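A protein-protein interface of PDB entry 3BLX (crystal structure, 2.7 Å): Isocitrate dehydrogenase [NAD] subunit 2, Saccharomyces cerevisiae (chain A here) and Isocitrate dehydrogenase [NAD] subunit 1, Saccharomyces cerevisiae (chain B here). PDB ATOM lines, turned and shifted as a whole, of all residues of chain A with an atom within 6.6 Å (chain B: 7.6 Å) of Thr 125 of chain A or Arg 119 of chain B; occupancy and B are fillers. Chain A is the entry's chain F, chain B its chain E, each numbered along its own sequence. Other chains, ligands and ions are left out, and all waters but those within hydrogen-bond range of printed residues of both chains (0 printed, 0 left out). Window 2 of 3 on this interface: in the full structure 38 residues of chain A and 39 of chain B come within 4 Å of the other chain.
Of the 15 printed residues of chain B, 6 touch a printed residue of chain A. Hydrophobic or aromatic side chains of chain A within 4 Å of the printed part of chain B: Tyr 126 and Val 229. Among the printed residues, 12 pairs touch across the chains.
The backbone carbonyl oxygen of Val 224 of chain B lies within hydrogen-bond range of the side-chain hydroxyl of Tyr 126 of chain A, 3.0 Å away. The backbone carbonyl oxygen (O) of Thr 230 of chain A lies within hydrogen-bond range of the guanidinium group (NH2) of Arg 119 of chain B, 2.6 Å away.
OG1 of Thr 124 of chain A is in hydrogen-bond range of O of Tyr 126 of chain A (2.9 Å).
Thr 125 of chain A touches Arg 119 of chain B. Tyr 126 of chain A touches Arg 119 of chain B. Tyr 126 of chain A touches Leu 250 of chain B. NH2 of Arg 119 of chain B touches O of Val 229 of chain A (3.6 Å). CG2 of Val 229 of chain A touches CG1 of Val 224 of chain B, at 3.7 Å. CG1 of Val 229 of chain A touches CB of Ala 249 of chain B (3.6 Å). Ala 249 of chain B touches Thr 230 of chain A. Gly 256 of chain A touches Val 224 of chain B (C to CG2, 3.7 Å). CA of Gly 260 of chain A touches CB of Ala 225 of chain B, at 3.8 Å. Gly 260 of chain A touches Lys 226 of chain B (O to NZ, 3.7 Å).
Of chain B, only Arg 119 (3.4 Å) comes within 4 Å of Thr 125 of chain A. Of the printed residues of chain A, Arg 119 of chain B touches Thr 125 (3.4 Å), Tyr 126 (3.4 Å), Val 229 (3.6 Å) and Thr 230 (2.6 Å). Of the printed residues of chain A, Ala 225 of chain B touches Gly 260. Of the printed residues of chain A, Lys 226 of chain B touches Gly 260. The nearest residue of chain A that does not touch Arg 119 of chain B is Pro 232 of chain A (4.03 Å).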
ATOM      1  N   LYS A 123      -8.757 -35.550 -12.697  1.00  0.00           N
ATOM      2  CA  LYS A 123      -8.251 -34.666 -11.653  1.00  0.00           C
ATOM      3  C   LYS A 123      -7.788 -33.327 -12.219  1.00  0.00           C
ATOM      4  O   LYS A 123      -6.748 -33.244 -12.881  1.00  0.00           O
ATOM      5  CB  LYS A 123      -7.089 -35.343 -10.915  1.00  0.00           C
ATOM      6  CG  LYS A 123      -6.471 -34.533  -9.773  1.00  0.00           C
ATOM      7  CD  LYS A 123      -7.353 -34.555  -8.523  1.00  0.00           C
ATOM      8  CE  LYS A 123      -6.644 -33.930  -7.316  1.00  0.00           C
ATOM      9  NZ  LYS A 123      -6.343 -32.477  -7.506  1.00  0.00           N
ATOM     10  N   THR A 124      -8.575 -32.288 -11.959  1.00  0.00           N
ATOM     11  CA  THR A 124      -8.188 -30.915 -12.271  1.00  0.00           C
ATOM     12  C   THR A 124      -8.091 -30.151 -10.964  1.00  0.00           C
ATOM     13  O   THR A 124      -8.523 -30.643  -9.921  1.00  0.00           O
ATOM     14  CB  THR A 124      -9.203 -30.218 -13.198  1.00  0.00           C
ATOM     15  OG1 THR A 124     -10.503 -30.220 -12.583  1.00  0.00           O
ATOM     16  CG2 THR A 124      -9.261 -30.925 -14.567  1.00  0.00           C
ATOM     17  N   THR A 125      -7.533 -28.950 -11.009  1.00  0.00           N
ATOM     18  CA  THR A 125      -7.238 -28.238  -9.775  1.00  0.00           C
ATOM     19  C   THR A 125      -8.491 -27.799  -8.984  1.00  0.00           C
ATOM     20  O   THR A 125      -8.467 -27.770  -7.746  1.00  0.00           O
ATOM     21  CB  THR A 125      -6.202 -27.101  -9.991  1.00  0.00           C
ATOM     22  OG1 THR A 125      -6.440 -26.057  -9.037  1.00  0.00           O
ATOM     23  CG2 THR A 125      -6.261 -26.539 -11.419  1.00  0.00           C
ATOM     24  N   TYR A 126      -9.588 -27.505  -9.686  1.00  0.00           N
ATOM     25  CA  TYR A 126     -10.874 -27.228  -9.027  1.00  0.00           C
ATOM     26  C   TYR A 126     -11.828 -28.412  -9.200  1.00  0.00           C
ATOM     27  O   TYR A 126     -11.750 -29.143 -10.194  1.00  0.00           O
ATOM     28  CB  TYR A 126     -11.527 -25.937  -9.560  1.00  0.00           C
ATOM     29  CG  TYR A 126     -10.772 -24.672  -9.195  1.00  0.00           C
ATOM     30  CD1 TYR A 126     -11.149 -23.888  -8.098  1.00  0.00           C
ATOM     31  CD2 TYR A 126      -9.668 -24.269  -9.944  1.00  0.00           C
ATOM     32  CE1 TYR A 126     -10.443 -22.724  -7.757  1.00  0.00           C
ATOM     33  CE2 TYR A 126      -8.959 -23.116  -9.609  1.00  0.00           C
ATOM     34  CZ  TYR A 126      -9.353 -22.355  -8.519  1.00  0.00           C
ATOM     35  OH  TYR A 126      -8.650 -21.229  -8.204  1.00  0.00           O
ATOM     36  N   GLU A 127     -12.736 -28.599  -8.245  1.00  0.00           N
ATOM     37  CA  GLU A 127     -13.619 -29.765  -8.278  1.00  0.00           C
ATOM     38  C   GLU A 127     -15.083 -29.428  -8.105  1.00  0.00           C
ATOM     39  O   GLU A 127     -15.435 -28.444  -7.456  1.00  0.00           O
ATOM     40  CB  GLU A 127     -13.203 -30.768  -7.205  1.00  0.00           C
ATOM     41  CG  GLU A 127     -11.747 -31.199  -7.336  1.00  0.00           C
ATOM     42  CD  GLU A 127     -11.412 -32.437  -6.523  1.00  0.00           C
ATOM     43  OE1 GLU A 127     -12.258 -32.865  -5.707  1.00  0.00           O
ATOM     44  OE2 GLU A 127     -10.296 -32.980  -6.703  1.00  0.00           O
ATOM     45  N   VAL A 228     -17.486 -17.549  -6.618  1.00  0.00           N
ATOM     46  CA  VAL A 228     -17.273 -18.643  -7.573  1.00  0.00           C
ATOM     47  C   VAL A 228     -15.863 -19.234  -7.520  1.00  0.00           C
ATOM     48  O   VAL A 228     -15.692 -20.418  -7.737  1.00  0.00           O
ATOM     49  CB  VAL A 228     -17.547 -18.205  -9.041  1.00  0.00           C
ATOM     50  CG1 VAL A 228     -17.358 -19.373  -9.987  1.00  0.00           C
ATOM     51  CG2 VAL A 228     -18.951 -17.652  -9.195  1.00  0.00           C
ATOM     52  N   VAL A 229     -14.847 -18.423  -7.252  1.00  0.00           N
ATOM     53  CA  VAL A 229     -13.498 -18.965  -7.242  1.00  0.00           C
ATOM     54  C   VAL A 229     -13.191 -19.677  -5.927  1.00  0.00           C
ATOM     55  O   VAL A 229     -12.472 -20.689  -5.914  1.00  0.00           O
ATOM     56  CB  VAL A 229     -12.437 -17.896  -7.557  1.00  0.00           C
ATOM     57  CG1 VAL A 229     -11.032 -18.428  -7.280  1.00  0.00           C
ATOM     58  CG2 VAL A 229     -12.594 -17.394  -9.016  1.00  0.00           C
ATOM     59  N   THR A 230     -13.727 -19.172  -4.818  1.00  0.00           N
ATOM     60  CA  THR A 230     -13.461 -19.826  -3.528  1.00  0.00           C
ATOM     61  C   THR A 230     -14.276 -21.118  -3.476  1.00  0.00           C
ATOM     62  O   THR A 230     -13.820 -22.128  -2.945  1.00  0.00           O
ATOM     63  CB  THR A 230     -13.753 -18.946  -2.264  1.00  0.00           C
ATOM     64  OG1 THR A 230     -15.017 -18.304  -2.403  1.00  0.00           O
ATOM     65  CG2 THR A 230     -12.691 -17.875  -2.055  1.00  0.00           C
ATOM     66  N   ASN A 231     -15.474 -21.092  -4.049  1.00  0.00           N
ATOM     67  CA  ASN A 231     -16.339 -22.266  -4.028  1.00  0.00           C
ATOM     68  C   ASN A 231     -17.271 -22.439  -5.254  1.00  0.00           C
ATOM     69  O   ASN A 231     -18.447 -22.056  -5.203  1.00  0.00           O
ATOM     70  CB  ASN A 231     -17.157 -22.285  -2.733  1.00  0.00           C
ATOM     71  CG  ASN A 231     -18.058 -23.508  -2.649  1.00  0.00           C
ATOM     72  OD1 ASN A 231     -17.777 -24.545  -3.269  1.00  0.00           O
ATOM     73  ND2 ASN A 231     -19.154 -23.391  -1.914  1.00  0.00           N
ATOM     74  N   PRO A 232     -16.751 -23.027  -6.344  1.00  0.00           N
ATOM     75  CA  PRO A 232     -17.527 -23.133  -7.589  1.00  0.00           C
ATOM     76  C   PRO A 232     -18.901 -23.812  -7.413  1.00  0.00           C
ATOM     77  O   PRO A 232     -19.884 -23.416  -8.060  1.00  0.00           O
ATOM     78  CB  PRO A 232     -16.616 -23.974  -8.495  1.00  0.00           C
ATOM     79  CG  PRO A 232     -15.226 -23.755  -7.961  1.00  0.00           C
ATOM     80  CD  PRO A 232     -15.387 -23.572  -6.478  1.00  0.00           C
ATOM     81  N   GLY A 256     -11.671 -21.684 -16.767  1.00  0.00           N
ATOM     82  CA  GLY A 256     -10.420 -21.818 -16.037  1.00  0.00           C
ATOM     83  C   GLY A 256     -10.642 -22.624 -14.779  1.00  0.00           C
ATOM     84  O   GLY A 256      -9.751 -23.359 -14.327  1.00  0.00           O
ATOM     85  N   LEU A 257     -11.838 -22.486 -14.212  1.00  0.00           N
ATOM     86  CA  LEU A 257     -12.224 -23.259 -13.034  1.00  0.00           C
ATOM     87  C   LEU A 257     -12.451 -24.743 -13.379  1.00  0.00           C
ATOM     88  O   LEU A 257     -11.888 -25.659 -12.756  1.00  0.00           O
ATOM     89  CB  LEU A 257     -13.476 -22.665 -12.381  1.00  0.00           C
ATOM     90  CG  LEU A 257     -13.338 -21.317 -11.658  1.00  0.00           C
ATOM     91  CD1 LEU A 257     -14.673 -20.861 -11.102  1.00  0.00           C
ATOM     92  CD2 LEU A 257     -12.307 -21.335 -10.545  1.00  0.00           C
ATOM     93  N   SER A 258     -13.272 -24.970 -14.392  1.00  0.00           N
ATOM     94  CA  SER A 258     -13.639 -26.318 -14.820  1.00  0.00           C
ATOM     95  C   SER A 258     -12.498 -27.129 -15.441  1.00  0.00           C
ATOM     96  O   SER A 258     -12.425 -28.339 -15.223  1.00  0.00           O
ATOM     97  CB  SER A 258     -14.836 -26.274 -15.778  1.00  0.00           C
ATOM     98  OG  SER A 258     -14.473 -25.654 -16.999  1.00  0.00           O
ATOM     99  N   ALA A 259     -11.600 -26.485 -16.185  1.00  0.00           N
ATOM    100  CA  ALA A 259     -10.575 -27.228 -16.915  1.00  0.00           C
ATOM    101  C   ALA A 259      -9.161 -26.645 -16.872  1.00  0.00           C
ATOM    102  O   ALA A 259      -8.180 -27.382 -17.016  1.00  0.00           O
ATOM    103  CB  ALA A 259     -11.013 -27.416 -18.358  1.00  0.00           C
ATOM    104  N   GLY A 260      -9.049 -25.328 -16.705  1.00  0.00           N
ATOM    105  CA  GLY A 260      -7.755 -24.663 -16.817  1.00  0.00           C
ATOM    106  C   GLY A 260      -7.400 -24.268 -18.250  1.00  0.00           C
ATOM    107  O   GLY A 260      -6.239 -23.989 -18.576  1.00  0.00           O
ATOM    108  N   VAL B 116      -2.994 -20.355   6.360  1.00  0.00           N
ATOM    109  CA  VAL B 116      -4.332 -20.286   5.778  1.00  0.00           C
ATOM    110  C   VAL B 116      -4.534 -21.345   4.691  1.00  0.00           C
ATOM    111  O   VAL B 116      -3.804 -21.375   3.697  1.00  0.00           O
ATOM    112  CB  VAL B 116      -4.654 -18.886   5.221  1.00  0.00           C
ATOM    113  CG1 VAL B 116      -6.014 -18.872   4.564  1.00  0.00           C
ATOM    114  CG2 VAL B 116      -4.667 -17.905   6.322  1.00  0.00           C
ATOM    115  N   LYS B 117      -5.532 -22.209   4.895  1.00  0.00           N
ATOM    116  CA  LYS B 117      -5.815 -23.306   3.965  1.00  0.00           C
ATOM    117  C   LYS B 117      -6.339 -22.794   2.619  1.00  0.00           C
ATOM    118  O   LYS B 117      -7.480 -22.324   2.519  1.00  0.00           O
ATOM    119  CB  LYS B 117      -6.794 -24.310   4.597  1.00  0.00           C
ATOM    120  CG  LYS B 117      -7.758 -23.666   5.586  1.00  0.00           C
ATOM    121  CD  LYS B 117      -8.759 -24.661   6.196  1.00  0.00           C
ATOM    122  CE  LYS B 117      -9.658 -23.951   7.234  1.00  0.00           C
ATOM    123  NZ  LYS B 117     -10.815 -24.764   7.738  1.00  0.00           N
ATOM    124  N   THR B 118      -5.490 -22.886   1.591  1.00  0.00           N
ATOM    125  CA  THR B 118      -5.852 -22.434   0.248  1.00  0.00           C
ATOM    126  C   THR B 118      -5.623 -23.517  -0.804  1.00  0.00           C
ATOM    127  O   THR B 118      -4.661 -24.287  -0.743  1.00  0.00           O
ATOM    128  CB  THR B 118      -5.075 -21.168  -0.175  1.00  0.00           C
ATOM    129  OG1 THR B 118      -3.666 -21.415  -0.105  1.00  0.00           O
ATOM    130  CG2 THR B 118      -5.431 -19.990   0.728  1.00  0.00           C
ATOM    131  N   ARG B 119      -6.512 -23.556  -1.785  1.00  0.00           N
ATOM    132  CA  ARG B 119      -6.447 -24.540  -2.855  1.00  0.00           C
ATOM    133  C   ARG B 119      -5.168 -24.424  -3.699  1.00  0.00           C
ATOM    134  O   ARG B 119      -4.637 -25.424  -4.181  1.00  0.00           O
ATOM    135  CB  ARG B 119      -7.725 -24.440  -3.689  1.00  0.00           C
ATOM    136  CG  ARG B 119      -7.744 -25.209  -4.969  1.00  0.00           C
ATOM    137  CD  ARG B 119      -9.178 -25.505  -5.381  1.00  0.00           C
ATOM    138  NE  ARG B 119     -10.102 -24.496  -4.876  1.00  0.00           N
ATOM    139  CZ  ARG B 119     -11.380 -24.726  -4.573  1.00  0.00           C
ATOM    140  NH1 ARG B 119     -11.909 -25.942  -4.714  1.00  0.00           N
ATOM    141  NH2 ARG B 119     -12.128 -23.731  -4.111  1.00  0.00           N
ATOM    142  N   ILE B 120      -4.654 -23.210  -3.858  1.00  0.00           N
ATOM    143  CA  ILE B 120      -3.365 -23.014  -4.512  1.00  0.00           C
ATOM    144  C   ILE B 120      -2.424 -22.263  -3.598  1.00  0.00           C
ATOM    145  O   ILE B 120      -2.721 -21.157  -3.157  1.00  0.00           O
ATOM    146  CB  ILE B 120      -3.503 -22.255  -5.828  1.00  0.00           C
ATOM    147  CG1 ILE B 120      -4.491 -22.989  -6.726  1.00  0.00           C
ATOM    148  CG2 ILE B 120      -2.130 -22.103  -6.498  1.00  0.00           C
ATOM    149  CD1 ILE B 120      -4.650 -22.394  -8.084  1.00  0.00           C
ATOM    150  N   PRO B 121      -1.280 -22.871  -3.306  1.00  0.00           N
ATOM    151  CA  PRO B 121      -0.342 -22.372  -2.298  1.00  0.00           C
ATOM    152  C   PRO B 121       0.631 -21.322  -2.848  1.00  0.00           C
ATOM    153  O   PRO B 121       0.822 -21.228  -4.067  1.00  0.00           O
ATOM    154  CB  PRO B 121       0.449 -23.634  -1.908  1.00  0.00           C
ATOM    155  CG  PRO B 121      -0.106 -24.766  -2.774  1.00  0.00           C
ATOM    156  CD  PRO B 121      -0.833 -24.140  -3.897  1.00  0.00           C
ATOM    157  N   ILE B 123       1.141 -17.863  -3.218  1.00  0.00           N
ATOM    158  CA  ILE B 123       0.819 -16.879  -4.229  1.00  0.00           C
ATOM    159  C   ILE B 123       1.483 -15.564  -3.861  1.00  0.00           C
ATOM    160  O   ILE B 123       1.593 -15.209  -2.670  1.00  0.00           O
ATOM    161  CB  ILE B 123      -0.696 -16.720  -4.372  1.00  0.00           C
ATOM    162  CG1 ILE B 123      -1.257 -17.932  -5.120  1.00  0.00           C
ATOM    163  CG2 ILE B 123      -1.049 -15.445  -5.122  1.00  0.00           C
ATOM    164  CD1 ILE B 123      -2.735 -18.044  -5.046  1.00  0.00           C
ATOM    165  N   VAL B 224      -6.821 -18.040 -12.231  1.00  0.00           N
ATOM    166  CA  VAL B 224      -7.429 -19.042 -11.369  1.00  0.00           C
ATOM    167  C   VAL B 224      -6.766 -20.404 -11.534  1.00  0.00           C
ATOM    168  O   VAL B 224      -6.805 -21.215 -10.611  1.00  0.00           O
ATOM    169  CB  VAL B 224      -8.957 -19.172 -11.579  1.00  0.00           C
ATOM    170  CG1 VAL B 224      -9.645 -17.864 -11.264  1.00  0.00           C
ATOM    171  CG2 VAL B 224      -9.293 -19.619 -12.997  1.00  0.00           C
ATOM    172  N   ALA B 225      -6.146 -20.639 -12.699  1.00  0.00           N
ATOM    173  CA  ALA B 225      -5.526 -21.933 -13.003  1.00  0.00           C
ATOM    174  C   ALA B 225      -4.023 -21.990 -12.701  1.00  0.00           C
ATOM    175  O   ALA B 225      -3.553 -22.978 -12.151  1.00  0.00           O
ATOM    176  CB  ALA B 225      -5.803 -22.345 -14.448  1.00  0.00           C
ATOM    177  N   LYS B 226      -3.274 -20.949 -13.061  1.00  0.00           N
ATOM    178  CA  LYS B 226      -1.820 -20.936 -12.837  1.00  0.00           C
ATOM    179  C   LYS B 226      -1.314 -19.544 -12.443  1.00  0.00           C
ATOM    180  O   LYS B 226      -0.553 -18.913 -13.181  1.00  0.00           O
ATOM    181  CB  LYS B 226      -1.051 -21.448 -14.067  1.00  0.00           C
ATOM    182  CG  LYS B 226      -1.719 -22.596 -14.847  1.00  0.00           C
ATOM    183  CD  LYS B 226      -0.845 -23.066 -16.035  1.00  0.00           C
ATOM    184  CE  LYS B 226      -1.682 -23.410 -17.287  1.00  0.00           C
ATOM    185  NZ  LYS B 226      -2.855 -24.314 -17.023  1.00  0.00           N
ATOM    186  N   PRO B 227      -1.719 -19.083 -11.260  1.00  0.00           N
ATOM    187  CA  PRO B 227      -1.403 -17.762 -10.715  1.00  0.00           C
ATOM    188  C   PRO B 227       0.085 -17.488 -10.610  1.00  0.00           C
ATOM    189  O   PRO B 227       0.457 -16.321 -10.469  1.00  0.00           O
ATOM    190  CB  PRO B 227      -1.963 -17.833  -9.297  1.00  0.00           C
ATOM    191  CG  PRO B 227      -2.971 -18.890  -9.320  1.00  0.00           C
ATOM    192  CD  PRO B 227      -2.511 -19.890 -10.322  1.00  0.00           C
ATOM    193  N   ALA B 249      -9.756 -14.290  -3.599  1.00  0.00           N
ATOM    194  CA  ALA B 249     -10.132 -15.693  -3.449  1.00  0.00           C
ATOM    195  C   ALA B 249      -8.911 -16.612  -3.359  1.00  0.00           C
ATOM    196  O   ALA B 249      -8.834 -17.451  -2.454  1.00  0.00           O
ATOM    197  CB  ALA B 249     -11.064 -16.136  -4.555  1.00  0.00           C
ATOM    198  N   LEU B 250      -7.957 -16.448  -4.277  1.00  0.00           N
ATOM    199  CA  LEU B 250      -6.700 -17.222  -4.257  1.00  0.00           C
ATOM    200  C   LEU B 250      -5.956 -17.329  -2.894  1.00  0.00           C
ATOM    201  O   LEU B 250      -5.332 -18.354  -2.623  1.00  0.00           O
ATOM    202  CB  LEU B 250      -5.738 -16.669  -5.307  1.00  0.00           C
ATOM    203  CG  LEU B 250      -5.656 -17.284  -6.697  1.00  0.00           C
ATOM    204  CD1 LEU B 250      -6.916 -18.031  -7.084  1.00  0.00           C
ATOM    205  CD2 LEU B 250      -5.374 -16.160  -7.659  1.00  0.00           C
ATOM    206  N   ILE B 251      -6.001 -16.282  -2.056  1.00  0.00           N
ATOM    207  CA  ILE B 251      -5.207 -16.266  -0.824  1.00  0.00           C
ATOM    208  C   ILE B 251      -6.053 -16.421   0.436  1.00  0.00           C
ATOM    209  O   ILE B 251      -5.537 -16.331   1.549  1.00  0.00           O
ATOM    210  CB  ILE B 251      -4.366 -14.965  -0.670  1.00  0.00           C
ATOM    211  CG1 ILE B 251      -5.280 -13.735  -0.646  1.00  0.00           C
ATOM    212  CG2 ILE B 251      -3.304 -14.854  -1.746  1.00  0.00           C
ATOM    213  CD1 ILE B 251      -4.744 -12.577   0.190  1.00  0.00           C
ATOM    214  N   GLY B 252      -7.353 -16.614   0.269  1.00  0.00           N
ATOM    215  CA  GLY B 252      -8.216 -16.886   1.400  1.00  0.00           C
ATOM    216  C   GLY B 252      -9.226 -15.810   1.767  1.00  0.00           C
ATOM    217  O   GLY B 252      -9.805 -15.830   2.861  1.00  0.00           O
